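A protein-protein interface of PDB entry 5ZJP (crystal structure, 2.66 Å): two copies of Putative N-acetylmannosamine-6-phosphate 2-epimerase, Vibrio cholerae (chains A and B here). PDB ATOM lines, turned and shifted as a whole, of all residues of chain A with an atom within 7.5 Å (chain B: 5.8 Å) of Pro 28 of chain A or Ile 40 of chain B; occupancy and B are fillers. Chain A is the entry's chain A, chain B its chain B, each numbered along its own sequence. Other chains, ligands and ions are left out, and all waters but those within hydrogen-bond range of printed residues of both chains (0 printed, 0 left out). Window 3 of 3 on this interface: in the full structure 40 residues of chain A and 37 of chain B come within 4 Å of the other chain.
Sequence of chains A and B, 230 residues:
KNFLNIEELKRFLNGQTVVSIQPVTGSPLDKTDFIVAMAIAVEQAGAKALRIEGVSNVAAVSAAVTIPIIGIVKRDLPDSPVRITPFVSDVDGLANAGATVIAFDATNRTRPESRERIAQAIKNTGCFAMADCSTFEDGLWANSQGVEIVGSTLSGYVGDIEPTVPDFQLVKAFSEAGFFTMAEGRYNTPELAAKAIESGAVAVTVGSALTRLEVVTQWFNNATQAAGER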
ATOM      1  N   PRO A  23       4.957  18.166  -1.223  1.00  0.00           N
ATOM      2  CA  PRO A  23       3.555  17.770  -1.413  1.00  0.00           C
ATOM      3  C   PRO A  23       3.017  18.210  -2.767  1.00  0.00           C
ATOM      4  O   PRO A  23       3.610  19.021  -3.481  1.00  0.00           O
ATOM      5  CB  PRO A  23       2.831  18.477  -0.263  1.00  0.00           C
ATOM      6  CG  PRO A  23       3.888  18.671   0.775  1.00  0.00           C
ATOM      7  CD  PRO A  23       5.137  18.970  -0.003  1.00  0.00           C
ATOM      8  N   VAL A  24       1.860  17.645  -3.118  1.00  0.00           N
ATOM      9  CA  VAL A  24       1.202  18.013  -4.364  1.00  0.00           C
ATOM     10  C   VAL A  24       0.788  19.478  -4.312  1.00  0.00           C
ATOM     11  O   VAL A  24       0.292  19.970  -3.290  1.00  0.00           O
ATOM     12  CB  VAL A  24      -0.011  17.100  -4.612  1.00  0.00           C
ATOM     13  CG1 VAL A  24      -0.676  17.429  -5.942  1.00  0.00           C
ATOM     14  CG2 VAL A  24       0.407  15.634  -4.557  1.00  0.00           C
ATOM     15  N   THR A  25       1.001  20.185  -5.420  1.00  0.00           N
ATOM     16  CA  THR A  25       0.694  21.608  -5.476  1.00  0.00           C
ATOM     17  C   THR A  25      -0.816  21.820  -5.481  1.00  0.00           C
ATOM     18  O   THR A  25      -1.546  21.146  -6.216  1.00  0.00           O
ATOM     19  CB  THR A  25       1.330  22.239  -6.714  1.00  0.00           C
ATOM     20  OG1 THR A  25       2.756  22.117  -6.632  1.00  0.00           O
ATOM     21  CG2 THR A  25       0.968  23.713  -6.812  1.00  0.00           C
ATOM     22  N   GLY A  26      -1.286  22.758  -4.658  1.00  0.00           N
ATOM     23  CA  GLY A  26      -2.703  22.993  -4.484  1.00  0.00           C
ATOM     24  C   GLY A  26      -3.378  22.084  -3.483  1.00  0.00           C
ATOM     25  O   GLY A  26      -4.549  22.312  -3.153  1.00  0.00           O
ATOM     26  N   SER A  27      -2.682  21.064  -2.991  1.00  0.00           N
ATOM     27  CA  SER A  27      -3.267  20.126  -2.053  1.00  0.00           C
ATOM     28  C   SER A  27      -3.497  20.795  -0.699  1.00  0.00           C
ATOM     29  O   SER A  27      -2.818  21.766  -0.353  1.00  0.00           O
ATOM     30  CB  SER A  27      -2.349  18.916  -1.884  1.00  0.00           C
ATOM     31  OG  SER A  27      -2.756  18.094  -0.806  1.00  0.00           O
ATOM     32  N   PRO A  28      -4.466  20.307   0.080  1.00  0.00           N
ATOM     33  CA  PRO A  28      -4.557  20.735   1.485  1.00  0.00           C
ATOM     34  C   PRO A  28      -3.288  20.456   2.268  1.00  0.00           C
ATOM     35  O   PRO A  28      -3.075  21.065   3.323  1.00  0.00           O
ATOM     36  CB  PRO A  28      -5.743  19.922   2.024  1.00  0.00           C
ATOM     37  CG  PRO A  28      -6.555  19.599   0.814  1.00  0.00           C
ATOM     38  CD  PRO A  28      -5.565  19.402  -0.294  1.00  0.00           C
ATOM     39  N   LEU A  29      -2.444  19.550   1.779  1.00  0.00           N
ATOM     40  CA  LEU A  29      -1.191  19.179   2.417  1.00  0.00           C
ATOM     41  C   LEU A  29      -0.022  20.046   1.968  1.00  0.00           C
ATOM     42  O   LEU A  29       1.094  19.863   2.466  1.00  0.00           O
ATOM     43  CB  LEU A  29      -0.879  17.708   2.121  1.00  0.00           C
ATOM     44  CG  LEU A  29      -1.932  16.693   2.575  1.00  0.00           C
ATOM     45  CD1 LEU A  29      -1.619  15.312   2.020  1.00  0.00           C
ATOM     46  CD2 LEU A  29      -2.039  16.657   4.091  1.00  0.00           C
ATOM     47  N   ASP A  30      -0.247  20.976   1.044  1.00  0.00           N
ATOM     48  CA  ASP A  30       0.812  21.819   0.492  1.00  0.00           C
ATOM     49  C   ASP A  30       1.023  23.077   1.333  1.00  0.00           C
ATOM     50  O   ASP A  30       1.036  24.197   0.824  1.00  0.00           O
ATOM     51  CB  ASP A  30       0.481  22.176  -0.954  1.00  0.00           C
ATOM     52  CG  ASP A  30       1.661  22.782  -1.695  1.00  0.00           C
ATOM     53  OD1 ASP A  30       2.788  22.741  -1.162  1.00  0.00           O
ATOM     54  OD2 ASP A  30       1.457  23.307  -2.810  1.00  0.00           O
ATOM     55  N   LYS A  31       1.199  22.898   2.639  1.00  0.00           N
ATOM     56  CA  LYS A  31       1.367  24.013   3.557  1.00  0.00           C
ATOM     57  C   LYS A  31       2.648  23.848   4.363  1.00  0.00           C
ATOM     58  O   LYS A  31       3.058  22.732   4.695  1.00  0.00           O
ATOM     59  CB  LYS A  31       0.162  24.147   4.493  1.00  0.00           C
ATOM     60  CG  LYS A  31      -1.111  24.507   3.753  1.00  0.00           C
ATOM     61  CD  LYS A  31      -0.901  25.772   2.936  1.00  0.00           C
ATOM     62  CE  LYS A  31      -2.066  26.036   2.001  1.00  0.00           C
ATOM     63  NZ  LYS A  31      -1.866  27.285   1.212  1.00  0.00           N
ATOM     64  N   PHE A  34       2.559  21.695   7.659  1.00  0.00           N
ATOM     65  CA  PHE A  34       2.583  20.251   7.447  1.00  0.00           C
ATOM     66  C   PHE A  34       3.920  19.795   6.876  1.00  0.00           C
ATOM     67  O   PHE A  34       4.351  18.666   7.139  1.00  0.00           O
ATOM     68  CB  PHE A  34       1.431  19.832   6.533  1.00  0.00           C
ATOM     69  CG  PHE A  34       1.126  18.360   6.579  1.00  0.00           C
ATOM     70  CD1 PHE A  34       0.432  17.817   7.647  1.00  0.00           C
ATOM     71  CD2 PHE A  34       1.523  17.523   5.552  1.00  0.00           C
ATOM     72  CE1 PHE A  34       0.146  16.464   7.694  1.00  0.00           C
ATOM     73  CE2 PHE A  34       1.241  16.167   5.592  1.00  0.00           C
ATOM     74  CZ  PHE A  34       0.551  15.638   6.665  1.00  0.00           C
ATOM     75  N   LEU A 213       0.543  12.030  -0.833  1.00  0.00           N
ATOM     76  CA  LEU A 213      -0.537  11.116  -0.472  1.00  0.00           C
ATOM     77  C   LEU A 213      -1.500  10.890  -1.634  1.00  0.00           C
ATOM     78  O   LEU A 213      -1.945   9.759  -1.864  1.00  0.00           O
ATOM     79  CB  LEU A 213      -1.280  11.650   0.753  1.00  0.00           C
ATOM     80  CG  LEU A 213      -2.380  10.762   1.333  1.00  0.00           C
ATOM     81  CD1 LEU A 213      -1.808   9.425   1.769  1.00  0.00           C
ATOM     82  CD2 LEU A 213      -3.056  11.458   2.501  1.00  0.00           C
ATOM     83  N   GLU A 214      -1.845  11.953  -2.367  1.00  0.00           N
ATOM     84  CA  GLU A 214      -2.719  11.801  -3.530  1.00  0.00           C
ATOM     85  C   GLU A 214      -2.129  10.833  -4.548  1.00  0.00           C
ATOM     86  O   GLU A 214      -2.834   9.967  -5.080  1.00  0.00           O
ATOM     87  CB  GLU A 214      -2.991  13.161  -4.181  1.00  0.00           C
ATOM     88  CG  GLU A 214      -3.856  14.115  -3.366  1.00  0.00           C
ATOM     89  CD  GLU A 214      -3.076  14.917  -2.345  1.00  0.00           C
ATOM     90  OE1 GLU A 214      -1.936  14.529  -2.012  1.00  0.00           O
ATOM     91  OE2 GLU A 214      -3.607  15.948  -1.880  1.00  0.00           O
ATOM     92  N   ILE B  35      -4.942  15.366  10.290  1.00  0.00           N
ATOM     93  CA  ILE B  35      -5.737  14.207   9.893  1.00  0.00           C
ATOM     94  C   ILE B  35      -6.851  14.626   8.940  1.00  0.00           C
ATOM     95  O   ILE B  35      -7.081  13.984   7.908  1.00  0.00           O
ATOM     96  CB  ILE B  35      -6.291  13.485  11.136  1.00  0.00           C
ATOM     97  CG1 ILE B  35      -5.153  12.839  11.927  1.00  0.00           C
ATOM     98  CG2 ILE B  35      -7.325  12.445  10.738  1.00  0.00           C
ATOM     99  CD1 ILE B  35      -5.575  12.290  13.273  1.00  0.00           C
ATOM    100  N   VAL B  36      -7.565  15.704   9.276  1.00  0.00           N
ATOM    101  CA  VAL B  36      -8.629  16.199   8.405  1.00  0.00           C
ATOM    102  C   VAL B  36      -8.069  16.596   7.044  1.00  0.00           C
ATOM    103  O   VAL B  36      -8.663  16.292   6.001  1.00  0.00           O
ATOM    104  CB  VAL B  36      -9.368  17.371   9.077  1.00  0.00           C
ATOM    105  CG1 VAL B  36     -10.401  17.958   8.131  1.00  0.00           C
ATOM    106  CG2 VAL B  36     -10.029  16.910  10.367  1.00  0.00           C
ATOM    107  N   ALA B  37      -6.925  17.284   7.032  1.00  0.00           N
ATOM    108  CA  ALA B  37      -6.286  17.657   5.772  1.00  0.00           C
ATOM    109  C   ALA B  37      -5.985  16.428   4.924  1.00  0.00           C
ATOM    110  O   ALA B  37      -6.230  16.416   3.713  1.00  0.00           O
ATOM    111  CB  ALA B  37      -5.010  18.452   6.046  1.00  0.00           C
ATOM    112  N   MET B  38      -5.435  15.383   5.549  1.00  0.00           N
ATOM    113  CA  MET B  38      -5.189  14.133   4.837  1.00  0.00           C
ATOM    114  C   MET B  38      -6.494  13.523   4.339  1.00  0.00           C
ATOM    115  O   MET B  38      -6.548  12.961   3.238  1.00  0.00           O
ATOM    116  CB  MET B  38      -4.448  13.155   5.749  1.00  0.00           C
ATOM    117  CG  MET B  38      -3.051  13.617   6.143  1.00  0.00           C
ATOM    118  SD  MET B  38      -2.120  12.405   7.103  1.00  0.00           S
ATOM    119  CE  MET B  38      -1.563  11.296   5.815  1.00  0.00           C
ATOM    120  N   ALA B  39      -7.557  13.619   5.142  1.00  0.00           N
ATOM    121  CA  ALA B  39      -8.858  13.094   4.735  1.00  0.00           C
ATOM    122  C   ALA B  39      -9.398  13.842   3.523  1.00  0.00           C
ATOM    123  O   ALA B  39      -9.877  13.228   2.562  1.00  0.00           O
ATOM    124  CB  ALA B  39      -9.842  13.172   5.901  1.00  0.00           C
ATOM    125  N   ILE B  40      -9.352  15.175   3.565  1.00  0.00           N
ATOM    126  CA  ILE B  40      -9.758  15.978   2.414  1.00  0.00           C
ATOM    127  C   ILE B  40      -8.944  15.593   1.184  1.00  0.00           C
ATOM    128  O   ILE B  40      -9.464  15.559   0.062  1.00  0.00           O
ATOM    129  CB  ILE B  40      -9.625  17.477   2.739  1.00  0.00           C
ATOM    130  CG1 ILE B  40     -10.622  17.870   3.828  1.00  0.00           C
ATOM    131  CG2 ILE B  40      -9.875  18.318   1.500  1.00  0.00           C
ATOM    132  CD1 ILE B  40     -10.441  19.279   4.329  1.00  0.00           C
ATOM    133  N   ALA B  41      -7.665  15.270   1.379  1.00  0.00           N
ATOM    134  CA  ALA B  41      -6.776  15.028   0.248  1.00  0.00           C
ATOM    135  C   ALA B  41      -7.118  13.723  -0.463  1.00  0.00           C
ATOM    136  O   ALA B  41      -7.188  13.680  -1.697  1.00  0.00           O
ATOM    137  CB  ALA B  41      -5.322  15.019   0.722  1.00  0.00           C
ATOM    138  N   VAL B  42      -7.331  12.642   0.295  1.00  0.00           N
ATOM    139  CA  VAL B  42      -7.625  11.358  -0.337  1.00  0.00           C
ATOM    140  C   VAL B  42      -8.988  11.382  -1.018  1.00  0.00           C
ATOM    141  O   VAL B  42      -9.184  10.725  -2.047  1.00  0.00           O
ATOM    142  CB  VAL B  42      -7.527  10.211   0.686  1.00  0.00           C
ATOM    143  CG1 VAL B  42      -6.095  10.043   1.157  1.00  0.00           C
ATOM    144  CG2 VAL B  42      -8.440  10.471   1.867  1.00  0.00           C
ATOM    145  N   GLU B  43      -9.950  12.125  -0.463  1.00  0.00           N
ATOM    146  CA  GLU B  43     -11.225  12.313  -1.146  1.00  0.00           C
ATOM    147  C   GLU B  43     -11.018  12.999  -2.489  1.00  0.00           C
ATOM    148  O   GLU B  43     -11.581  12.585  -3.509  1.00  0.00           O
ATOM    149  CB  GLU B  43     -12.179  13.121  -0.269  1.00  0.00           C
ATOM    150  CG  GLU B  43     -13.626  13.076  -0.731  1.00  0.00           C
ATOM    151  CD  GLU B  43     -14.534  13.952   0.108  1.00  0.00           C
ATOM    152  OE1 GLU B  43     -14.043  14.961   0.658  1.00  0.00           O
ATOM    153  OE2 GLU B  43     -15.733  13.623   0.230  1.00  0.00           O
ATOM    154  N   GLN B  44     -10.214  14.065  -2.500  1.00  0.00           N
ATOM    155  CA  GLN B  44      -9.895  14.761  -3.741  1.00  0.00           C
ATOM    156  C   GLN B  44      -9.180  13.848  -4.727  1.00  0.00           C
ATOM    157  O   GLN B  44      -9.360  13.985  -5.943  1.00  0.00           O
ATOM    158  CB  GLN B  44      -9.037  15.987  -3.431  1.00  0.00           C
ATOM    159  CG  GLN B  44      -9.761  17.084  -2.666  1.00  0.00           C
ATOM    160  CD  GLN B  44      -8.821  18.177  -2.198  1.00  0.00           C
ATOM    161  OE1 GLN B  44      -7.602  18.009  -2.219  1.00  0.00           O
ATOM    162  NE2 GLN B  44      -9.382  19.303  -1.771  1.00  0.00           N
ATOM    163  N   ALA B  45      -8.369  12.916  -4.229  1.00  0.00           N
ATOM    164  CA  ALA B  45      -7.642  11.980  -5.079  1.00  0.00           C
ATOM    165  C   ALA B  45      -8.457  10.752  -5.473  1.00  0.00           C
ATOM    166  O   ALA B  45      -7.933   9.895  -6.194  1.00  0.00           O
ATOM    167  CB  ALA B  45      -6.353  11.536  -4.381  1.00  0.00           C
ATOM    168  N   ALA B  64     -15.976  17.477   7.171  1.00  0.00           N
ATOM    169  CA  ALA B  64     -15.145  18.049   6.124  1.00  0.00           C
ATOM    170  C   ALA B  64     -15.088  17.223   4.847  1.00  0.00           C
ATOM    171  O   ALA B  64     -14.737  17.773   3.799  1.00  0.00           O
ATOM    172  CB  ALA B  64     -13.709  18.258   6.632  1.00  0.00           C
ATOM    173  N   VAL B  65     -15.419  15.933   4.896  1.00  0.00           N
ATOM    174  CA  VAL B  65     -15.469  15.110   3.693  1.00  0.00           C
ATOM    175  C   VAL B  65     -16.883  14.575   3.511  1.00  0.00           C
ATOM    176  O   VAL B  65     -17.761  14.814   4.348  1.00  0.00           O
ATOM    177  CB  VAL B  65     -14.439  13.966   3.742  1.00  0.00           C
ATOM    178  CG1 VAL B  65     -13.028  14.526   3.896  1.00  0.00           C
ATOM    179  CG2 VAL B  65     -14.770  12.988   4.856  1.00  0.00           C
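Printed residues of chain A within 4 Å of Val 42 of chain B: Leu 213.
Printed residues of chain B within 4 Å of Glu 214 of chain A: Ala 41 and Ala 45.
Printed residues of chain A within 4 Å of Gln 44 of chain B: Pro 28 (3.1 Å).
Asp 30 of chain A touches none of the printed residues of chain B.
The nearest residue of chain A that does not touch Ile 40 of chain B is Glu 214 of chain A (6.2 Å).
No position is printed for both chains.
Of the 10 pairs that touch across the chains among the printed residues, none has its exchanged pair printed and touching as well.
The backbone NH (N) of Leu 29 of chain A lies close to the side-chain hydroxyl (OG) of Ser 27 of chain A, at 3.0 Å.
The side-chain hydroxyl (OG) of Ser 27 of chain A is in hydrogen-bond range of the side-chain carboxylate (OE2) of Glu 214 of chain A, 2.5 Å away.
Pro 28 of chain A touches Ala 37 of chain B (CB to O, 3.9 Å).
Pro 28 of chain A touches Ile 40 of chain B.
Gln 44 of chain B touches Pro 28 of chain A (OE1 to CD, 3.1 Å).
CB of Ala 37 of chain B touches CD2 of Leu 29 of chain A, 3.98 Å away.
CG of Met 38 of chain B touches CD2 of Leu 29 of chain A, at 3.8 Å.
Ala 41 of chain B touches Leu 29 of chain A.
CD2 of Leu 213 of chain A touches CE of Met 38 of chain B, 3.6 Å away.
Leu 213 of chain A touches Val 42 of chain B (CD2 to CG1, 3.6 Å).
CB of Ala 41 of chain B touches OE2 of Glu 214 of chain A (3.3 Å).
Glu 214 of chain A touches Ala 45 of chain B (CG to CB, 3.7 Å).
Printed residues of chain B that touch a printed residue of chain A: Ala 37, Met 38, Ile 40, Ala 41, Val 42, Gln 44 and Ala 45.
Hydrophobic or aromatic side chains of chain B within 4 Å of the printed part of chain A: Ala 37, Met 38, Ile 40, Ala 41, Val 42 and Ala 45.
Of the 12 printed residues of chain A, 4 touch a printed residue of chain B.
Printed residues of chain A that touch a printed residue of chain B: Pro 28, Leu 29, Leu 213 and Glu 214.
Hydrophobic or aromatic side chains of chain A within 4 Å of the printed part of chain B: Pro 28, Leu 29 and Leu 213.
Among the printed residues, 10 pairs touch across the chains.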
